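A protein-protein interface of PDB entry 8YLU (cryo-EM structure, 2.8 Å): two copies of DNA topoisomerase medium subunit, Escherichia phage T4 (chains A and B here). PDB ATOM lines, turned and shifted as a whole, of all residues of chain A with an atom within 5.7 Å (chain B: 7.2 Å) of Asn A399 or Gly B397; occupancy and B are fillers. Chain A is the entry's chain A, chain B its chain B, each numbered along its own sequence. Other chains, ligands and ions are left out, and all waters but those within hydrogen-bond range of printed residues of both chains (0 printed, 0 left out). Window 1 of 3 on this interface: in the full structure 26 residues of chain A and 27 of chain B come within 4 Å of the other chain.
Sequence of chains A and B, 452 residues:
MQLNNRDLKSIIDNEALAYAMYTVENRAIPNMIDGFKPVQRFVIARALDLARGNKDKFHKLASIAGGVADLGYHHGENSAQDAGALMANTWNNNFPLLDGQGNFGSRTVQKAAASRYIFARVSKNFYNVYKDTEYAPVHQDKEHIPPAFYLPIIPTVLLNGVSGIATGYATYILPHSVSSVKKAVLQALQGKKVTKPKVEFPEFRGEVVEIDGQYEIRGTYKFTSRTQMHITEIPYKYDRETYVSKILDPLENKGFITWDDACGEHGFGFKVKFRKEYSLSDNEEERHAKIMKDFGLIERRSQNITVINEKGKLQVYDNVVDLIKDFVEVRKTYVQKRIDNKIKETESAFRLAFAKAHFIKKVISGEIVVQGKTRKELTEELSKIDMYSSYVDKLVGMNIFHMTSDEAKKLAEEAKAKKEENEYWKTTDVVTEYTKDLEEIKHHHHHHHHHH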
ATOM      1  N   GLY A 397       7.773  26.733 -18.608  1.00  0.00           N
ATOM      2  CA  GLY A 397       7.097  25.645 -19.281  1.00  0.00           C
ATOM      3  C   GLY A 397       8.013  24.469 -19.547  1.00  0.00           C
ATOM      4  O   GLY A 397       7.718  23.625 -20.397  1.00  0.00           O
ATOM      5  N   MET A 398       9.131  24.409 -18.830  1.00  0.00           N
ATOM      6  CA  MET A 398      10.096  23.334 -18.996  1.00  0.00           C
ATOM      7  C   MET A 398       9.833  22.222 -17.990  1.00  0.00           C
ATOM      8  O   MET A 398       9.358  22.462 -16.878  1.00  0.00           O
ATOM      9  CB  MET A 398      11.521  23.859 -18.839  1.00  0.00           C
ATOM     10  CG  MET A 398      11.800  25.115 -19.643  1.00  0.00           C
ATOM     11  SD  MET A 398      13.511  25.670 -19.546  1.00  0.00           S
ATOM     12  CE  MET A 398      14.250  24.323 -18.636  1.00  0.00           C
ATOM     13  N   ASN A 399      10.157  20.996 -18.391  1.00  0.00           N
ATOM     14  CA  ASN A 399       9.819  19.827 -17.598  1.00  0.00           C
ATOM     15  C   ASN A 399      10.713  19.726 -16.362  1.00  0.00           C
ATOM     16  O   ASN A 399      11.708  20.439 -16.212  1.00  0.00           O
ATOM     17  CB  ASN A 399       9.931  18.561 -18.444  1.00  0.00           C
ATOM     18  CG  ASN A 399       9.036  18.600 -19.664  1.00  0.00           C
ATOM     19  OD1 ASN A 399       9.096  19.536 -20.461  1.00  0.00           O
ATOM     20  ND2 ASN A 399       8.194  17.586 -19.814  1.00  0.00           N
ATOM     21  N   ILE A 400      10.326  18.824 -15.456  1.00  0.00           N
ATOM     22  CA  ILE A 400      11.060  18.643 -14.208  1.00  0.00           C
ATOM     23  C   ILE A 400      12.446  18.069 -14.476  1.00  0.00           C
ATOM     24  O   ILE A 400      13.437  18.499 -13.872  1.00  0.00           O
ATOM     25  CB  ILE A 400      10.254  17.757 -13.241  1.00  0.00           C
ATOM     26  CG1 ILE A 400       9.065  18.530 -12.665  1.00  0.00           C
ATOM     27  CG2 ILE A 400      11.146  17.209 -12.135  1.00  0.00           C
ATOM     28  CD1 ILE A 400       9.339  19.200 -11.339  1.00  0.00           C
ATOM     29  N   PHE A 401      12.546  17.106 -15.396  1.00  0.00           N
ATOM     30  CA  PHE A 401      13.819  16.433 -15.630  1.00  0.00           C
ATOM     31  C   PHE A 401      14.887  17.365 -16.186  1.00  0.00           C
ATOM     32  O   PHE A 401      16.066  16.996 -16.186  1.00  0.00           O
ATOM     33  CB  PHE A 401      13.621  15.221 -16.553  1.00  0.00           C
ATOM     34  CG  PHE A 401      12.950  15.537 -17.867  1.00  0.00           C
ATOM     35  CD1 PHE A 401      11.729  14.966 -18.178  1.00  0.00           C
ATOM     36  CD2 PHE A 401      13.553  16.356 -18.807  1.00  0.00           C
ATOM     37  CE1 PHE A 401      11.108  15.235 -19.381  1.00  0.00           C
ATOM     38  CE2 PHE A 401      12.937  16.627 -20.010  1.00  0.00           C
ATOM     39  CZ  PHE A 401      11.714  16.064 -20.299  1.00  0.00           C
ATOM     40  N   HIS A 402      14.511  18.559 -16.649  1.00  0.00           N
ATOM     41  CA  HIS A 402      15.498  19.548 -17.061  1.00  0.00           C
ATOM     42  C   HIS A 402      16.342  20.048 -15.898  1.00  0.00           C
ATOM     43  O   HIS A 402      17.366  20.696 -16.132  1.00  0.00           O
ATOM     44  CB  HIS A 402      14.810  20.730 -17.744  1.00  0.00           C
ATOM     45  CG  HIS A 402      14.369  20.443 -19.145  1.00  0.00           C
ATOM     46  ND1 HIS A 402      13.400  21.183 -19.786  1.00  0.00           N
ATOM     47  CD2 HIS A 402      14.763  19.494 -20.027  1.00  0.00           C
ATOM     48  CE1 HIS A 402      13.216  20.703 -21.003  1.00  0.00           C
ATOM     49  NE2 HIS A 402      14.031  19.678 -21.174  1.00  0.00           N
ATOM     50  N   MET A 403      15.937  19.771 -14.660  1.00  0.00           N
ATOM     51  CA  MET A 403      16.733  20.113 -13.491  1.00  0.00           C
ATOM     52  C   MET A 403      17.688  18.999 -13.083  1.00  0.00           C
ATOM     53  O   MET A 403      18.388  19.141 -12.076  1.00  0.00           O
ATOM     54  CB  MET A 403      15.818  20.470 -12.315  1.00  0.00           C
ATOM     55  CG  MET A 403      14.999  21.733 -12.539  1.00  0.00           C
ATOM     56  SD  MET A 403      13.745  22.037 -11.279  1.00  0.00           S
ATOM     57  CE  MET A 403      14.337  21.016  -9.935  1.00  0.00           C
ATOM     58  N   PHE B 359       3.226  13.880  -5.582  1.00  0.00           N
ATOM     59  CA  PHE B 359       4.624  14.045  -5.957  1.00  0.00           C
ATOM     60  C   PHE B 359       5.035  15.508  -5.894  1.00  0.00           C
ATOM     61  O   PHE B 359       6.143  15.830  -5.450  1.00  0.00           O
ATOM     62  CB  PHE B 359       4.865  13.481  -7.356  1.00  0.00           C
ATOM     63  CG  PHE B 359       6.244  13.748  -7.891  1.00  0.00           C
ATOM     64  CD1 PHE B 359       7.357  13.196  -7.281  1.00  0.00           C
ATOM     65  CD2 PHE B 359       6.426  14.548  -9.006  1.00  0.00           C
ATOM     66  CE1 PHE B 359       8.625  13.439  -7.771  1.00  0.00           C
ATOM     67  CE2 PHE B 359       7.692  14.793  -9.501  1.00  0.00           C
ATOM     68  CZ  PHE B 359       8.791  14.237  -8.883  1.00  0.00           C
ATOM     69  N   VAL B 370      14.901  17.130  -6.867  1.00  0.00           N
ATOM     70  CA  VAL B 370      15.238  16.769  -8.241  1.00  0.00           C
ATOM     71  C   VAL B 370      16.686  17.122  -8.558  1.00  0.00           C
ATOM     72  O   VAL B 370      17.394  16.358  -9.224  1.00  0.00           O
ATOM     73  CB  VAL B 370      14.261  17.448  -9.217  1.00  0.00           C
ATOM     74  CG1 VAL B 370      14.569  17.045 -10.649  1.00  0.00           C
ATOM     75  CG2 VAL B 370      12.827  17.108  -8.853  1.00  0.00           C
ATOM     76  N   ARG B 375      19.360  11.452 -14.629  1.00  0.00           N
ATOM     77  CA  ARG B 375      18.038  11.048 -15.095  1.00  0.00           C
ATOM     78  C   ARG B 375      17.664   9.670 -14.562  1.00  0.00           C
ATOM     79  O   ARG B 375      16.549   9.463 -14.066  1.00  0.00           O
ATOM     80  CB  ARG B 375      18.002  11.059 -16.623  1.00  0.00           C
ATOM     81  CG  ARG B 375      16.648  10.722 -17.221  1.00  0.00           C
ATOM     82  CD  ARG B 375      15.719  11.920 -17.203  1.00  0.00           C
ATOM     83  NE  ARG B 375      14.513  11.676 -17.984  1.00  0.00           N
ATOM     84  CZ  ARG B 375      14.423  11.853 -19.295  1.00  0.00           C
ATOM     85  NH1 ARG B 375      15.456  12.268 -20.010  1.00  0.00           N
ATOM     86  NH2 ARG B 375      13.267  11.606 -19.905  1.00  0.00           N
ATOM     87  N   TYR B 391       3.889   5.565 -13.154  1.00  0.00           N
ATOM     88  CA  TYR B 391       3.589   6.948 -13.503  1.00  0.00           C
ATOM     89  C   TYR B 391       4.817   7.850 -13.458  1.00  0.00           C
ATOM     90  O   TYR B 391       4.674   9.075 -13.543  1.00  0.00           O
ATOM     91  CB  TYR B 391       2.507   7.503 -12.572  1.00  0.00           C
ATOM     92  CG  TYR B 391       1.233   6.689 -12.553  1.00  0.00           C
ATOM     93  CD1 TYR B 391       0.605   6.318 -13.734  1.00  0.00           C
ATOM     94  CD2 TYR B 391       0.669   6.277 -11.354  1.00  0.00           C
ATOM     95  CE1 TYR B 391      -0.557   5.570 -13.720  1.00  0.00           C
ATOM     96  CE2 TYR B 391      -0.490   5.528 -11.330  1.00  0.00           C
ATOM     97  CZ  TYR B 391      -1.099   5.178 -12.514  1.00  0.00           C
ATOM     98  OH  TYR B 391      -2.255   4.433 -12.495  1.00  0.00           O
ATOM     99  N   VAL B 392       6.018   7.280 -13.333  1.00  0.00           N
ATOM    100  CA  VAL B 392       7.215   8.095 -13.135  1.00  0.00           C
ATOM    101  C   VAL B 392       7.525   8.919 -14.381  1.00  0.00           C
ATOM    102  O   VAL B 392       7.974  10.069 -14.284  1.00  0.00           O
ATOM    103  CB  VAL B 392       8.400   7.202 -12.722  1.00  0.00           C
ATOM    104  CG1 VAL B 392       8.557   6.033 -13.686  1.00  0.00           C
ATOM    105  CG2 VAL B 392       9.682   8.015 -12.633  1.00  0.00           C
ATOM    106  N   ASP B 393       7.290   8.351 -15.567  1.00  0.00           N
ATOM    107  CA  ASP B 393       7.575   9.074 -16.804  1.00  0.00           C
ATOM    108  C   ASP B 393       6.742  10.346 -16.907  1.00  0.00           C
ATOM    109  O   ASP B 393       7.258  11.408 -17.273  1.00  0.00           O
ATOM    110  CB  ASP B 393       7.324   8.169 -18.010  1.00  0.00           C
ATOM    111  CG  ASP B 393       6.020   7.402 -17.903  1.00  0.00           C
ATOM    112  OD1 ASP B 393       5.614   7.068 -16.769  1.00  0.00           O
ATOM    113  OD2 ASP B 393       5.400   7.131 -18.952  1.00  0.00           O
ATOM    114  N   LYS B 394       5.452  10.258 -16.586  1.00  0.00           N
ATOM    115  CA  LYS B 394       4.601  11.440 -16.567  1.00  0.00           C
ATOM    116  C   LYS B 394       4.857  12.319 -15.353  1.00  0.00           C
ATOM    117  O   LYS B 394       4.550  13.515 -15.394  1.00  0.00           O
ATOM    118  CB  LYS B 394       3.129  11.027 -16.608  1.00  0.00           C
ATOM    119  CG  LYS B 394       2.725  10.348 -17.903  1.00  0.00           C
ATOM    120  CD  LYS B 394       1.219  10.209 -18.013  1.00  0.00           C
ATOM    121  CE  LYS B 394       0.826   8.784 -18.367  1.00  0.00           C
ATOM    122  NZ  LYS B 394       1.166   8.447 -19.776  1.00  0.00           N
ATOM    123  N   LEU B 395       5.406  11.755 -14.277  1.00  0.00           N
ATOM    124  CA  LEU B 395       5.723  12.550 -13.096  1.00  0.00           C
ATOM    125  C   LEU B 395       6.891  13.492 -13.363  1.00  0.00           C
ATOM    126  O   LEU B 395       6.837  14.678 -13.021  1.00  0.00           O
ATOM    127  CB  LEU B 395       6.034  11.628 -11.920  1.00  0.00           C
ATOM    128  CG  LEU B 395       5.037  11.607 -10.765  1.00  0.00           C
ATOM    129  CD1 LEU B 395       3.711  11.026 -11.210  1.00  0.00           C
ATOM    130  CD2 LEU B 395       5.614  10.802  -9.625  1.00  0.00           C
ATOM    131  N   VAL B 396       7.963  12.976 -13.970  1.00  0.00           N
ATOM    132  CA  VAL B 396       9.119  13.818 -14.263  1.00  0.00           C
ATOM    133  C   VAL B 396       8.890  14.704 -15.480  1.00  0.00           C
ATOM    134  O   VAL B 396       9.599  15.703 -15.650  1.00  0.00           O
ATOM    135  CB  VAL B 396      10.384  12.969 -14.471  1.00  0.00           C
ATOM    136  CG1 VAL B 396      10.724  12.206 -13.201  1.00  0.00           C
ATOM    137  CG2 VAL B 396      10.201  12.020 -15.644  1.00  0.00           C
ATOM    138  N   GLY B 397       7.924  14.371 -16.330  1.00  0.00           N
ATOM    139  CA  GLY B 397       7.619  15.172 -17.495  1.00  0.00           C
ATOM    140  C   GLY B 397       6.777  16.395 -17.232  1.00  0.00           C
ATOM    141  O   GLY B 397       6.505  17.161 -18.159  1.00  0.00           O
ATOM    142  N   MET B 398       6.349  16.597 -15.990  1.00  0.00           N
ATOM    143  CA  MET B 398       5.544  17.756 -15.646  1.00  0.00           C
ATOM    144  C   MET B 398       6.400  19.018 -15.629  1.00  0.00           C
ATOM    145  O   MET B 398       7.617  18.975 -15.438  1.00  0.00           O
ATOM    146  CB  MET B 398       4.869  17.543 -14.294  1.00  0.00           C
ATOM    147  CG  MET B 398       3.657  16.632 -14.367  1.00  0.00           C
ATOM    148  SD  MET B 398       2.949  16.271 -12.756  1.00  0.00           S
ATOM    149  CE  MET B 398       4.240  16.873 -11.687  1.00  0.00           C
ATOM    150  N   ASN B 399       5.742  20.155 -15.833  1.00  0.00           N
ATOM    151  CA  ASN B 399       6.445  21.408 -16.047  1.00  0.00           C
ATOM    152  C   ASN B 399       6.890  22.028 -14.725  1.00  0.00           C
ATOM    153  O   ASN B 399       6.446  21.647 -13.639  1.00  0.00           O
ATOM    154  CB  ASN B 399       5.565  22.379 -16.829  1.00  0.00           C
ATOM    155  CG  ASN B 399       5.027  21.770 -18.105  1.00  0.00           C
ATOM    156  OD1 ASN B 399       5.717  21.725 -19.123  1.00  0.00           O
ATOM    157  ND2 ASN B 399       3.792  21.290 -18.058  1.00  0.00           N
ATOM    158  N   ILE B 400       7.798  23.000 -14.835  1.00  0.00           N
ATOM    159  CA  ILE B 400       8.327  23.678 -13.654  1.00  0.00           C
ATOM    160  C   ILE B 400       7.233  24.474 -12.955  1.00  0.00           C
ATOM    161  O   ILE B 400       7.205  24.564 -11.721  1.00  0.00           O
ATOM    162  CB  ILE B 400       9.527  24.562 -14.045  1.00  0.00           C
ATOM    163  CG1 ILE B 400      10.768  23.702 -14.287  1.00  0.00           C
ATOM    164  CG2 ILE B 400       9.815  25.603 -12.980  1.00  0.00           C
ATOM    165  CD1 ILE B 400      11.935  24.470 -14.861  1.00  0.00           C
ATOM    166  N   HIS B 402       4.376  23.618 -12.393  1.00  0.00           N
ATOM    167  CA  HIS B 402       3.662  22.731 -11.486  1.00  0.00           C
ATOM    168  C   HIS B 402       4.465  22.546 -10.208  1.00  0.00           C
ATOM    169  O   HIS B 402       4.647  21.417  -9.747  1.00  0.00           O
ATOM    170  CB  HIS B 402       3.423  21.368 -12.137  1.00  0.00           C
ATOM    171  CG  HIS B 402       2.267  21.335 -13.085  1.00  0.00           C
ATOM    172  ND1 HIS B 402       1.239  22.251 -13.040  1.00  0.00           N
ATOM    173  CD2 HIS B 402       1.977  20.493 -14.105  1.00  0.00           C
ATOM    174  CE1 HIS B 402       0.365  21.974 -13.990  1.00  0.00           C
ATOM    175  NE2 HIS B 402       0.790  20.913 -14.652  1.00  0.00           N
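Printed residues of chain B within 4 Å of Asn A399: Gly B397 (2.4 Å), Met B398 (3.2 Å) and Ile B400 (3.9 Å).
Of the printed residues of chain B, Ile A400 touches Val B370, Val B396 and Met B398.
Of the printed residues of chain B, Phe A401 touches Arg B375 (3.9 Å), Val B396 (3.3 Å) and Gly B397 (3.97 Å).
Asp B393 touches none of the printed residues of chain A.
Gly B397 touches just these residues of chain A: Asn A399 (2.4 Å) and Phe A401 (3.97 Å).
Of the printed residues of chain A, Ile B400 touches Met A398 (2.6 Å) and Asn A399 (3.9 Å).
His B402 touches none of the printed residues of chain A.
The nearest residue of chain A that does not touch Gly B397 is Ile A400 (4.7 Å).
Gly A397 touches Asn B399, and with the chains exchanged Asn A399 touches Gly B397.
Met A398 touches Asn B399, and with the chains exchanged Asn A399 touches Met B398.
Met A398 touches Ile B400, and with the chains exchanged Ile A400 touches Met B398.
Asn A399 touches Ile B400, but with the chains exchanged Ile A400 does not touch Asn B399 (4.2 Å).
5 positions are printed for both chains.
The backbone carbonyl oxygen (O) of Gly A397 sits close to the side-chain amide oxygen (OD1) of Asn B399 (3.0 Å).
ND2 of Asn A399 is in hydrogen-bond range of O of Gly B397.
The backbone NH (N) of Phe A401 is in hydrogen-bond range of the backbone carbonyl oxygen (O) of Val B396.
N of Ile A400 is in hydrogen-bond range of O of Met B398, at 2.7 Å.
The backbone NH (N) of Ile A400 sits at hydrogen-bond distance from the backbone carbonyl oxygen (O) of Val B396.
The backbone NH of Ile B400 lies within hydrogen-bond range of the backbone carbonyl oxygen of Met A398 (2.6 Å).
Of the 7 printed residues of chain A, 6 touch a printed residue of chain B.
Printed residues of chain A that touch a printed residue of chain B: Gly A397, Met A398, Asn A399, Ile A400, Phe A401 and Met A403.
Hydrophobic or aromatic side chains of chain A that line the printed part of chain B: Ile A400, Phe A401 and Met A403.
Among the printed residues, 13 pairs touch across the chains.
Among the printed residues, no Asp or Glu carboxylate lies within 4 Å of a Lys or Arg side-chain nitrogen of the other chain.
Among the printed residues, merely in contact across the chains: Met A398 with Asn B399 (3.2 Å), Asn A399 with Met B398 (3.2 Å), Asn A399 with Ile B400 (3.9 Å), Ile A400 with Val B370 (3.7 Å), Phe A401 with Arg B375 (3.9 Å), Phe A401 with Gly B397 (3.97 Å) and Met A403 with Val B370 (3.6 Å).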
